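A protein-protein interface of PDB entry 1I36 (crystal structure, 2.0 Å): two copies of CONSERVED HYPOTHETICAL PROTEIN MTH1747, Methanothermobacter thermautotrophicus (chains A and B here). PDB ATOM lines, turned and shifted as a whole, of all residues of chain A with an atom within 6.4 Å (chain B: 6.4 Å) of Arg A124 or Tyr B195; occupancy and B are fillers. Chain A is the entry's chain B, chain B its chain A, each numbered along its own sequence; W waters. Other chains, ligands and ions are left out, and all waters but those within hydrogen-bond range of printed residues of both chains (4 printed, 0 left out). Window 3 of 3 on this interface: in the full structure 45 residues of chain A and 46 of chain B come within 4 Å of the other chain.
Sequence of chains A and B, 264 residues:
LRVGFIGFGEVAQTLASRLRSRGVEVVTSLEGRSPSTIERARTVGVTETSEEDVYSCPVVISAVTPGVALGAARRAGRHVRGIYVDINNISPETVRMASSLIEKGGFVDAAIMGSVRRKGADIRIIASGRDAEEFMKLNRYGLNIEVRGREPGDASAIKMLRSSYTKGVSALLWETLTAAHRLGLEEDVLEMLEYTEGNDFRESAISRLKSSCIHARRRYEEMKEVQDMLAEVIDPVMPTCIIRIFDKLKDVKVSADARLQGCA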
ATOM      1  N   ALA A 111       1.983  -3.255  17.315  1.00  0.00           N
ATOM      2  CA  ALA A 111       1.204  -3.361  16.077  1.00  0.00           C
ATOM      3  C   ALA A 111       2.073  -2.807  14.969  1.00  0.00           C
ATOM      4  O   ALA A 111       2.581  -1.703  15.092  1.00  0.00           O
ATOM      5  CB  ALA A 111      -0.116  -2.502  16.194  1.00  0.00           C
ATOM      6  N   ILE A 112       2.261  -3.577  13.908  1.00  0.00           N
ATOM      7  CA  ILE A 112       3.064  -3.146  12.775  1.00  0.00           C
ATOM      8  C   ILE A 112       2.191  -2.228  11.915  1.00  0.00           C
ATOM      9  O   ILE A 112       1.093  -2.609  11.491  1.00  0.00           O
ATOM     10  CB  ILE A 112       3.561  -4.368  11.961  1.00  0.00           C
ATOM     11  CG1 ILE A 112       4.598  -5.133  12.781  1.00  0.00           C
ATOM     12  CG2 ILE A 112       4.155  -3.909  10.626  1.00  0.00           C
ATOM     13  CD1 ILE A 112       4.836  -6.552  12.302  1.00  0.00           C
ATOM     14  N   MET A 113       2.687  -1.022  11.650  1.00  0.00           N
ATOM     15  CA  MET A 113       1.926  -0.038  10.888  1.00  0.00           C
ATOM     16  C   MET A 113       2.395   0.177   9.458  1.00  0.00           C
ATOM     17  O   MET A 113       2.519   1.305   8.999  1.00  0.00           O
ATOM     18  CB  MET A 113       1.914   1.294  11.638  1.00  0.00           C
ATOM     19  CG  MET A 113       1.397   1.197  13.068  1.00  0.00           C
ATOM     20  SD  MET A 113      -0.269   0.500  13.113  1.00  0.00           S
ATOM     21  CE  MET A 113      -1.279   1.911  12.614  1.00  0.00           C
ATOM     22  N   GLY A 114       2.614  -0.911   8.743  1.00  0.00           N
ATOM     23  CA  GLY A 114       3.053  -0.799   7.366  1.00  0.00           C
ATOM     24  C   GLY A 114       3.348  -2.170   6.812  1.00  0.00           C
ATOM     25  O   GLY A 114       3.002  -3.182   7.434  1.00  0.00           O
ATOM     26  N   LYS A 119       9.075  -2.008   3.577  1.00  0.00           N
ATOM     27  CA  LYS A 119       9.900  -1.186   4.464  1.00  0.00           C
ATOM     28  C   LYS A 119      10.975  -1.894   5.297  1.00  0.00           C
ATOM     29  O   LYS A 119      11.839  -1.246   5.870  1.00  0.00           O
ATOM     30  CB  LYS A 119       9.004  -0.336   5.377  1.00  0.00           C
ATOM     31  CG  LYS A 119       8.275   0.829   4.671  1.00  0.00           C
ATOM     32  CD  LYS A 119       7.284   0.329   3.611  1.00  0.00           C
ATOM     33  CE  LYS A 119       6.709   1.464   2.749  1.00  0.00           C
ATOM     34  NZ  LYS A 119       6.294   1.008   1.367  1.00  0.00           N
ATOM     35  N   GLY A 120      10.908  -3.211   5.407  1.00  0.00           N
ATOM     36  CA  GLY A 120      11.904  -3.917   6.201  1.00  0.00           C
ATOM     37  C   GLY A 120      11.832  -3.572   7.685  1.00  0.00           C
ATOM     38  O   GLY A 120      10.752  -3.249   8.199  1.00  0.00           O
ATOM     39  N   ALA A 121      12.984  -3.595   8.359  1.00  0.00           N
ATOM     40  CA  ALA A 121      13.042  -3.297   9.787  1.00  0.00           C
ATOM     41  C   ALA A 121      12.792  -1.830  10.119  1.00  0.00           C
ATOM     42  O   ALA A 121      12.691  -1.470  11.290  1.00  0.00           O
ATOM     43  CB  ALA A 121      14.348  -3.765  10.387  1.00  0.00           C
ATOM     44  N   ASP A 122      12.705  -0.985   9.097  1.00  0.00           N
ATOM     45  CA  ASP A 122      12.424   0.436   9.300  1.00  0.00           C
ATOM     46  C   ASP A 122      10.935   0.697   9.494  1.00  0.00           C
ATOM     47  O   ASP A 122      10.516   1.826   9.777  1.00  0.00           O
ATOM     48  CB  ASP A 122      12.933   1.248   8.116  1.00  0.00           C
ATOM     49  CG  ASP A 122      14.421   1.066   7.905  1.00  0.00           C
ATOM     50  OD1 ASP A 122      15.215   1.618   8.709  1.00  0.00           O
ATOM     51  OD2 ASP A 122      14.778   0.311   6.967  1.00  0.00           O
ATOM     52  N   ILE A 123      10.152  -0.371   9.396  1.00  0.00           N
ATOM     53  CA  ILE A 123       8.712  -0.298   9.562  1.00  0.00           C
ATOM     54  C   ILE A 123       8.361   0.347  10.912  1.00  0.00           C
ATOM     55  O   ILE A 123       9.020   0.080  11.917  1.00  0.00           O
ATOM     56  CB  ILE A 123       8.115  -1.734   9.492  1.00  0.00           C
ATOM     57  CG1 ILE A 123       6.619  -1.669   9.334  1.00  0.00           C
ATOM     58  CG2 ILE A 123       8.485  -2.564  10.704  1.00  0.00           C
ATOM     59  CD1 ILE A 123       6.248  -1.487   7.929  1.00  0.00           C
ATOM     60  N   ARG A 124       7.347   1.212  10.923  1.00  0.00           N
ATOM     61  CA  ARG A 124       6.899   1.849  12.155  1.00  0.00           C
ATOM     62  C   ARG A 124       6.105   0.846  13.011  1.00  0.00           C
ATOM     63  O   ARG A 124       5.232   0.160  12.505  1.00  0.00           O
ATOM     64  CB  ARG A 124       6.020   3.071  11.859  1.00  0.00           C
ATOM     65  CG  ARG A 124       5.385   3.693  13.110  1.00  0.00           C
ATOM     66  CD  ARG A 124       5.433   5.206  13.060  1.00  0.00           C
ATOM     67  NE  ARG A 124       6.822   5.679  13.077  1.00  0.00           N
ATOM     68  CZ  ARG A 124       7.330   6.462  14.024  1.00  0.00           C
ATOM     69  NH1 ARG A 124       6.553   6.872  15.027  1.00  0.00           N
ATOM     70  NH2 ARG A 124       8.623   6.797  14.001  1.00  0.00           N
ATOM     71  N   ILE A 125       6.492   0.687  14.272  1.00  0.00           N
ATOM     72  CA  ILE A 125       5.777  -0.222  15.176  1.00  0.00           C
ATOM     73  C   ILE A 125       5.235   0.574  16.351  1.00  0.00           C
ATOM     74  O   ILE A 125       5.992   1.300  16.983  1.00  0.00           O
ATOM     75  CB  ILE A 125       6.729  -1.308  15.759  1.00  0.00           C
ATOM     76  CG1 ILE A 125       7.328  -2.146  14.631  1.00  0.00           C
ATOM     77  CG2 ILE A 125       5.948  -2.240  16.716  1.00  0.00           C
ATOM     78  CD1 ILE A 125       8.389  -3.172  15.086  1.00  0.00           C
ATOM     79  N   ILE A 126       3.933   0.508  16.620  1.00  0.00           N
ATOM     80  CA  ILE A 126       3.414   1.213  17.798  1.00  0.00           C
ATOM     81  C   ILE A 126       3.223   0.168  18.904  1.00  0.00           C
ATOM     82  O   ILE A 126       2.927  -0.976  18.616  1.00  0.00           O
ATOM     83  CB  ILE A 126       2.121   2.005  17.517  1.00  0.00           C
ATOM     84  CG1 ILE A 126       1.025   1.076  16.991  1.00  0.00           C
ATOM     85  CG2 ILE A 126       2.441   3.142  16.462  1.00  0.00           C
ATOM     86  CD1 ILE A 126      -0.383   1.743  17.009  1.00  0.00           C
ATOM     87  N   ASN A 144      12.097   0.918  14.898  1.00  0.00           N
ATOM     88  CA  ASN A 144      11.347   2.153  14.789  1.00  0.00           C
ATOM     89  C   ASN A 144      10.033   2.037  15.569  1.00  0.00           C
ATOM     90  O   ASN A 144       8.933   2.039  14.988  1.00  0.00           O
ATOM     91  CB  ASN A 144      11.075   2.389  13.289  1.00  0.00           C
ATOM     92  CG  ASN A 144      10.463   3.735  13.013  1.00  0.00           C
ATOM     93  OD1 ASN A 144      10.360   4.578  13.904  1.00  0.00           O
ATOM     94  ND2 ASN A 144       9.985   3.926  11.784  1.00  0.00           N
ATOM     95  N   ILE A 145      10.154   2.020  16.895  1.00  0.00           N
ATOM     96  CA  ILE A 145       9.016   1.851  17.788  1.00  0.00           C
ATOM     97  C   ILE A 145       8.562   3.169  18.382  1.00  0.00           C
ATOM     98  O   ILE A 145       9.352   4.055  18.654  1.00  0.00           O
ATOM     99  CB  ILE A 145       9.385   0.897  18.953  1.00  0.00           C
ATOM    100  CG1 ILE A 145       9.776  -0.484  18.382  1.00  0.00           C
ATOM    101  CG2 ILE A 145       8.240   0.818  20.012  1.00  0.00           C
ATOM    102  CD1 ILE A 145      10.813  -1.174  19.245  1.00  0.00           C
ATOM    103  N   GLU A 146       7.271   3.265  18.612  1.00  0.00           N
ATOM    104  CA  GLU A 146       6.696   4.450  19.219  1.00  0.00           C
ATOM    105  C   GLU A 146       5.620   3.969  20.186  1.00  0.00           C
ATOM    106  O   GLU A 146       4.860   3.056  19.878  1.00  0.00           O
ATOM    107  CB  GLU A 146       6.128   5.306  18.093  1.00  0.00           C
ATOM    108  CG  GLU A 146       5.060   6.294  18.444  1.00  0.00           C
ATOM    109  CD  GLU A 146       4.587   7.024  17.187  1.00  0.00           C
ATOM    110  OE1 GLU A 146       5.146   8.103  16.893  1.00  0.00           O
ATOM    111  OE2 GLU A 146       3.698   6.498  16.477  1.00  0.00           O
ATOM    112  N   ARG A 148       2.170   4.296  22.171  1.00  0.00           N
ATOM    113  CA  ARG A 148       0.844   4.913  21.995  1.00  0.00           C
ATOM    114  C   ARG A 148      -0.118   4.324  23.011  1.00  0.00           C
ATOM    115  O   ARG A 148       0.165   3.269  23.575  1.00  0.00           O
ATOM    116  CB  ARG A 148       0.308   4.596  20.603  1.00  0.00           C
ATOM    117  CG  ARG A 148       1.188   5.098  19.482  1.00  0.00           C
ATOM    118  CD  ARG A 148       0.896   6.523  19.227  1.00  0.00           C
ATOM    119  NE  ARG A 148       1.586   7.042  18.051  1.00  0.00           N
ATOM    120  CZ  ARG A 148       1.328   8.238  17.539  1.00  0.00           C
ATOM    121  NH1 ARG A 148       0.381   8.985  18.075  1.00  0.00           N
ATOM    122  NH2 ARG A 148       2.148   8.765  16.639  1.00  0.00           N
ATOM    123  N   ARG A 162      -7.701   2.369  12.253  1.00  0.00           N
ATOM    124  CA  ARG A 162      -7.196   2.986  11.046  1.00  0.00           C
ATOM    125  C   ARG A 162      -7.618   2.136   9.840  1.00  0.00           C
ATOM    126  O   ARG A 162      -8.135   2.662   8.844  1.00  0.00           O
ATOM    127  CB  ARG A 162      -5.676   3.131  11.050  1.00  0.00           C
ATOM    128  CG  ARG A 162      -5.166   3.587   9.686  1.00  0.00           C
ATOM    129  CD  ARG A 162      -3.696   3.848   9.637  1.00  0.00           C
ATOM    130  NE  ARG A 162      -2.905   2.649   9.392  1.00  0.00           N
ATOM    131  CZ  ARG A 162      -1.582   2.654   9.219  1.00  0.00           C
ATOM    132  NH1 ARG A 162      -0.895   3.801   9.260  1.00  0.00           N
ATOM    133  NH2 ARG A 162      -0.942   1.517   8.984  1.00  0.00           N
ATOM    134  N   LEU B 190      -5.875   9.648  14.572  1.00  0.00           N
ATOM    135  CA  LEU B 190      -5.669  10.748  13.616  1.00  0.00           C
ATOM    136  C   LEU B 190      -4.233  10.828  13.117  1.00  0.00           C
ATOM    137  O   LEU B 190      -3.985  10.969  11.915  1.00  0.00           O
ATOM    138  CB  LEU B 190      -6.068  12.075  14.245  1.00  0.00           C
ATOM    139  CG  LEU B 190      -7.568  12.285  14.265  1.00  0.00           C
ATOM    140  CD1 LEU B 190      -7.967  13.390  15.249  1.00  0.00           C
ATOM    141  CD2 LEU B 190      -7.990  12.633  12.831  1.00  0.00           C
ATOM    142  N   GLU B 191      -3.270  10.677  14.026  1.00  0.00           N
ATOM    143  CA  GLU B 191      -1.862  10.728  13.618  1.00  0.00           C
ATOM    144  C   GLU B 191      -1.477   9.549  12.768  1.00  0.00           C
ATOM    145  O   GLU B 191      -0.647   9.676  11.852  1.00  0.00           O
ATOM    146  CB  GLU B 191      -0.930  10.803  14.823  1.00  0.00           C
ATOM    147  CG  GLU B 191      -0.976  12.140  15.558  1.00  0.00           C
ATOM    148  CD  GLU B 191      -0.026  12.168  16.751  1.00  0.00           C
ATOM    149  OE1 GLU B 191       1.076  11.581  16.631  1.00  0.00           O
ATOM    150  OE2 GLU B 191      -0.383  12.762  17.794  1.00  0.00           O
ATOM    151  N   MET B 192      -2.054   8.386  13.062  1.00  0.00           N
ATOM    152  CA  MET B 192      -1.734   7.208  12.263  1.00  0.00           C
ATOM    153  C   MET B 192      -2.318   7.395  10.882  1.00  0.00           C
ATOM    154  O   MET B 192      -1.690   7.022   9.906  1.00  0.00           O
ATOM    155  CB  MET B 192      -2.221   5.903  12.911  1.00  0.00           C
ATOM    156  CG  MET B 192      -1.326   5.427  14.061  1.00  0.00           C
ATOM    157  SD  MET B 192       0.489   5.477  13.735  1.00  0.00           S
ATOM    158  CE  MET B 192       0.858   6.879  14.608  1.00  0.00           C
ATOM    159  N   LEU B 193      -3.505   7.993  10.790  1.00  0.00           N
ATOM    160  CA  LEU B 193      -4.113   8.251   9.469  1.00  0.00           C
ATOM    161  C   LEU B 193      -3.297   9.238   8.617  1.00  0.00           C
ATOM    162  O   LEU B 193      -3.146   9.049   7.412  1.00  0.00           O
ATOM    163  CB  LEU B 193      -5.549   8.740   9.608  1.00  0.00           C
ATOM    164  CG  LEU B 193      -6.570   7.665   9.988  1.00  0.00           C
ATOM    165  CD1 LEU B 193      -7.845   8.323  10.433  1.00  0.00           C
ATOM    166  CD2 LEU B 193      -6.814   6.706   8.826  1.00  0.00           C
ATOM    167  N   GLU B 194      -2.743  10.282   9.215  1.00  0.00           N
ATOM    168  CA  GLU B 194      -1.946  11.172   8.384  1.00  0.00           C
ATOM    169  C   GLU B 194      -0.612  10.524   8.060  1.00  0.00           C
ATOM    170  O   GLU B 194      -0.012  10.800   7.034  1.00  0.00           O
ATOM    171  CB  GLU B 194      -1.780  12.553   9.012  1.00  0.00           C
ATOM    172  CG  GLU B 194      -1.050  12.627  10.322  1.00  0.00           C
ATOM    173  CD  GLU B 194      -0.932  14.065  10.820  1.00  0.00           C
ATOM    174  OE1 GLU B 194      -1.019  14.994   9.976  1.00  0.00           O
ATOM    175  OE2 GLU B 194      -0.748  14.258  12.049  1.00  0.00           O
ATOM    176  N   TYR B 195      -0.194   9.593   8.907  1.00  0.00           N
ATOM    177  CA  TYR B 195       1.053   8.872   8.712  1.00  0.00           C
ATOM    178  C   TYR B 195       0.886   7.895   7.548  1.00  0.00           C
ATOM    179  O   TYR B 195       1.855   7.277   7.124  1.00  0.00           O
ATOM    180  CB  TYR B 195       1.433   8.135  10.003  1.00  0.00           C
ATOM    181  CG  TYR B 195       2.779   7.451   9.967  1.00  0.00           C
ATOM    182  CD1 TYR B 195       3.958   8.182  10.118  1.00  0.00           C
ATOM    183  CD2 TYR B 195       2.876   6.068   9.754  1.00  0.00           C
ATOM    184  CE1 TYR B 195       5.195   7.558  10.057  1.00  0.00           C
ATOM    185  CE2 TYR B 195       4.113   5.435   9.688  1.00  0.00           C
ATOM    186  CZ  TYR B 195       5.265   6.189   9.842  1.00  0.00           C
ATOM    187  OH  TYR B 195       6.491   5.579   9.791  1.00  0.00           O
ATOM    188  N   THR B 196      -0.341   7.786   7.025  1.00  0.00           N
ATOM    189  CA  THR B 196      -0.671   6.895   5.900  1.00  0.00           C
ATOM    190  C   THR B 196      -1.427   7.572   4.746  1.00  0.00           C
ATOM    191  O   THR B 196      -1.191   7.240   3.585  1.00  0.00           O
ATOM    192  CB  THR B 196      -1.481   5.628   6.352  1.00  0.00           C
ATOM    193  OG1 THR B 196      -2.125   5.034   5.217  1.00  0.00           O
ATOM    194  CG2 THR B 196      -2.551   5.976   7.358  1.00  0.00           C
ATOM    195  N   GLU B 197      -2.349   8.486   5.055  1.00  0.00           N
ATOM    196  CA  GLU B 197      -3.125   9.183   4.020  1.00  0.00           C
ATOM    197  C   GLU B 197      -2.388  10.407   3.452  1.00  0.00           C
ATOM    198  O   GLU B 197      -3.007  11.310   2.880  1.00  0.00           O
ATOM    199  CB  GLU B 197      -4.512   9.595   4.542  1.00  0.00           C
ATOM    200  CG  GLU B 197      -5.343   8.456   5.148  1.00  0.00           C
ATOM    201  CD  GLU B 197      -5.414   7.213   4.263  1.00  0.00           C
ATOM    202  OE1 GLU B 197      -4.545   6.319   4.408  1.00  0.00           O
ATOM    203  OE2 GLU B 197      -6.348   7.124   3.440  1.00  0.00           O
ATOM    204  N   GLY B 198      -1.070  10.429   3.641  1.00  0.00           N
ATOM    205  CA  GLY B 198      -0.235  11.503   3.140  1.00  0.00           C
ATOM    206  C   GLY B 198      -0.576  12.918   3.554  1.00  0.00           C
ATOM    207  O   GLY B 198      -0.129  13.381   4.617  1.00  0.00           O
ATOM    208  N   PHE B 201      -4.038  15.505   6.190  1.00  0.00           N
ATOM    209  CA  PHE B 201      -5.152  14.733   6.748  1.00  0.00           C
ATOM    210  C   PHE B 201      -5.769  15.246   8.053  1.00  0.00           C
ATOM    211  O   PHE B 201      -6.931  15.677   8.064  1.00  0.00           O
ATOM    212  CB  PHE B 201      -4.796  13.249   6.895  1.00  0.00           C
ATOM    213  CG  PHE B 201      -5.979  12.384   7.229  1.00  0.00           C
ATOM    214  CD1 PHE B 201      -6.803  11.920   6.220  1.00  0.00           C
ATOM    215  CD2 PHE B 201      -6.341  12.137   8.552  1.00  0.00           C
ATOM    216  CE1 PHE B 201      -7.977  11.239   6.510  1.00  0.00           C
ATOM    217  CE2 PHE B 201      -7.523  11.456   8.848  1.00  0.00           C
ATOM    218  CZ  PHE B 201      -8.338  11.013   7.823  1.00  0.00           C
HETATM  219  O   HOH W   1      -3.501   2.960   6.527  1.00  0.00           O
HETATM  220  O   HOH W   2       3.037  11.043  14.817  1.00  0.00           O
HETATM  221  O   HOH W   3      -1.238  11.086  19.836  1.00  0.00           O
HETATM  222  O   HOH W   4       9.147   6.698  10.719  1.00  0.00           O
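The guanidinium group of Arg A148 is in salt-bridge range of the side-chain carboxylate of Glu B191 (3.0 Å). The backbone carbonyl oxygen (O) of Met B192 sits at hydrogen-bond distance from the guanidinium group (NH1) of Arg A162 (3.4 Å). The guanidinium group (NE) of Arg A124 lies close to the side-chain hydroxyl (OH) of Tyr B195, at 3.3 Å.
Hydrophobic or aromatic side chains of chain B within 4 Å of the printed part of chain A: Met B192, Leu B193 and Tyr B195. Of the 17 printed residues of chain A, 5 touch a printed residue of chain B. Printed residues of chain A that touch a printed residue of chain B: Met A113, Arg A124, Glu A146, Arg A148 and Arg A162. Hydrophobic or aromatic side chains of chain A within 4 Å of the printed part of chain B: Met A113. Among the printed residues, 8 pairs touch across the chains.
OG1 of Thr B196 sits at hydrogen-bond distance from OE1 of Glu B197, 2.9 Å away. O of Arg A124 lies within hydrogen-bond range of N of Met A113 (2.9 Å). The guanidinium group (NH2) of Arg A162 is in hydrogen-bond range of the backbone carbonyl oxygen (O) of Met A113 (3.5 Å). OD1 of Asn A144 lies within hydrogen-bond range of NH2 of Arg A124 (2.8 Å). The guanidinium group (NH1) of Arg A124 lies within salt-bridge range of the side-chain carboxylate (OE1) of Glu A146 (2.6 Å). The backbone carbonyl oxygen (O) of Ile A125 lies within hydrogen-bond range of the backbone NH (N) of Glu A146 (2.9 Å).
Water W2 lies within hydrogen-bond range of the side-chain carboxylate (OE1) of Glu B191 and the guanidinium group (NH2) of Arg A148. Water W3 lies within hydrogen-bond range of OE2 of Glu B191 (2.8 Å) and NH1 of Arg A148 (3.2 Å). Water W1 bridges OG1 of Thr B196 and NE of Arg A162. Water W4 lies within hydrogen-bond range of OH of Tyr B195, ND2 of Asn A144 and NH2 of Arg A124.
Gly A114 touches none of the printed residues of chain B. Arg A124 touches just one residue of chain B: Tyr B195 (3.3 Å). Of the printed residues of chain B, Glu A146 touches Met B192 (3.4 Å). Of the printed residues of chain B, Arg A148 touches Glu B191 and Met B192. Printed residues of chain A within 4 Å of Glu B191: Arg A148. Tyr B195 touches just one residue of chain A: Arg A124 (3.3 Å). Printed residues of chain A within 4 Å of Thr B196: Arg A162. The nearest printed residue of chain A that does not touch Leu B193 is Met A113 (6.7 Å).
No position is printed for both chains. Of the 8 pairs that touch across the chains among the printed residues, none has its exchanged pair printed and touching as well.
Among the printed residues, pairs that only touch across the chains: Met A113 with Met B192, Glu A146 with Met B192, Arg A148 with Met B192, Arg A162 with Leu B193 and Arg A162 with Thr B196.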
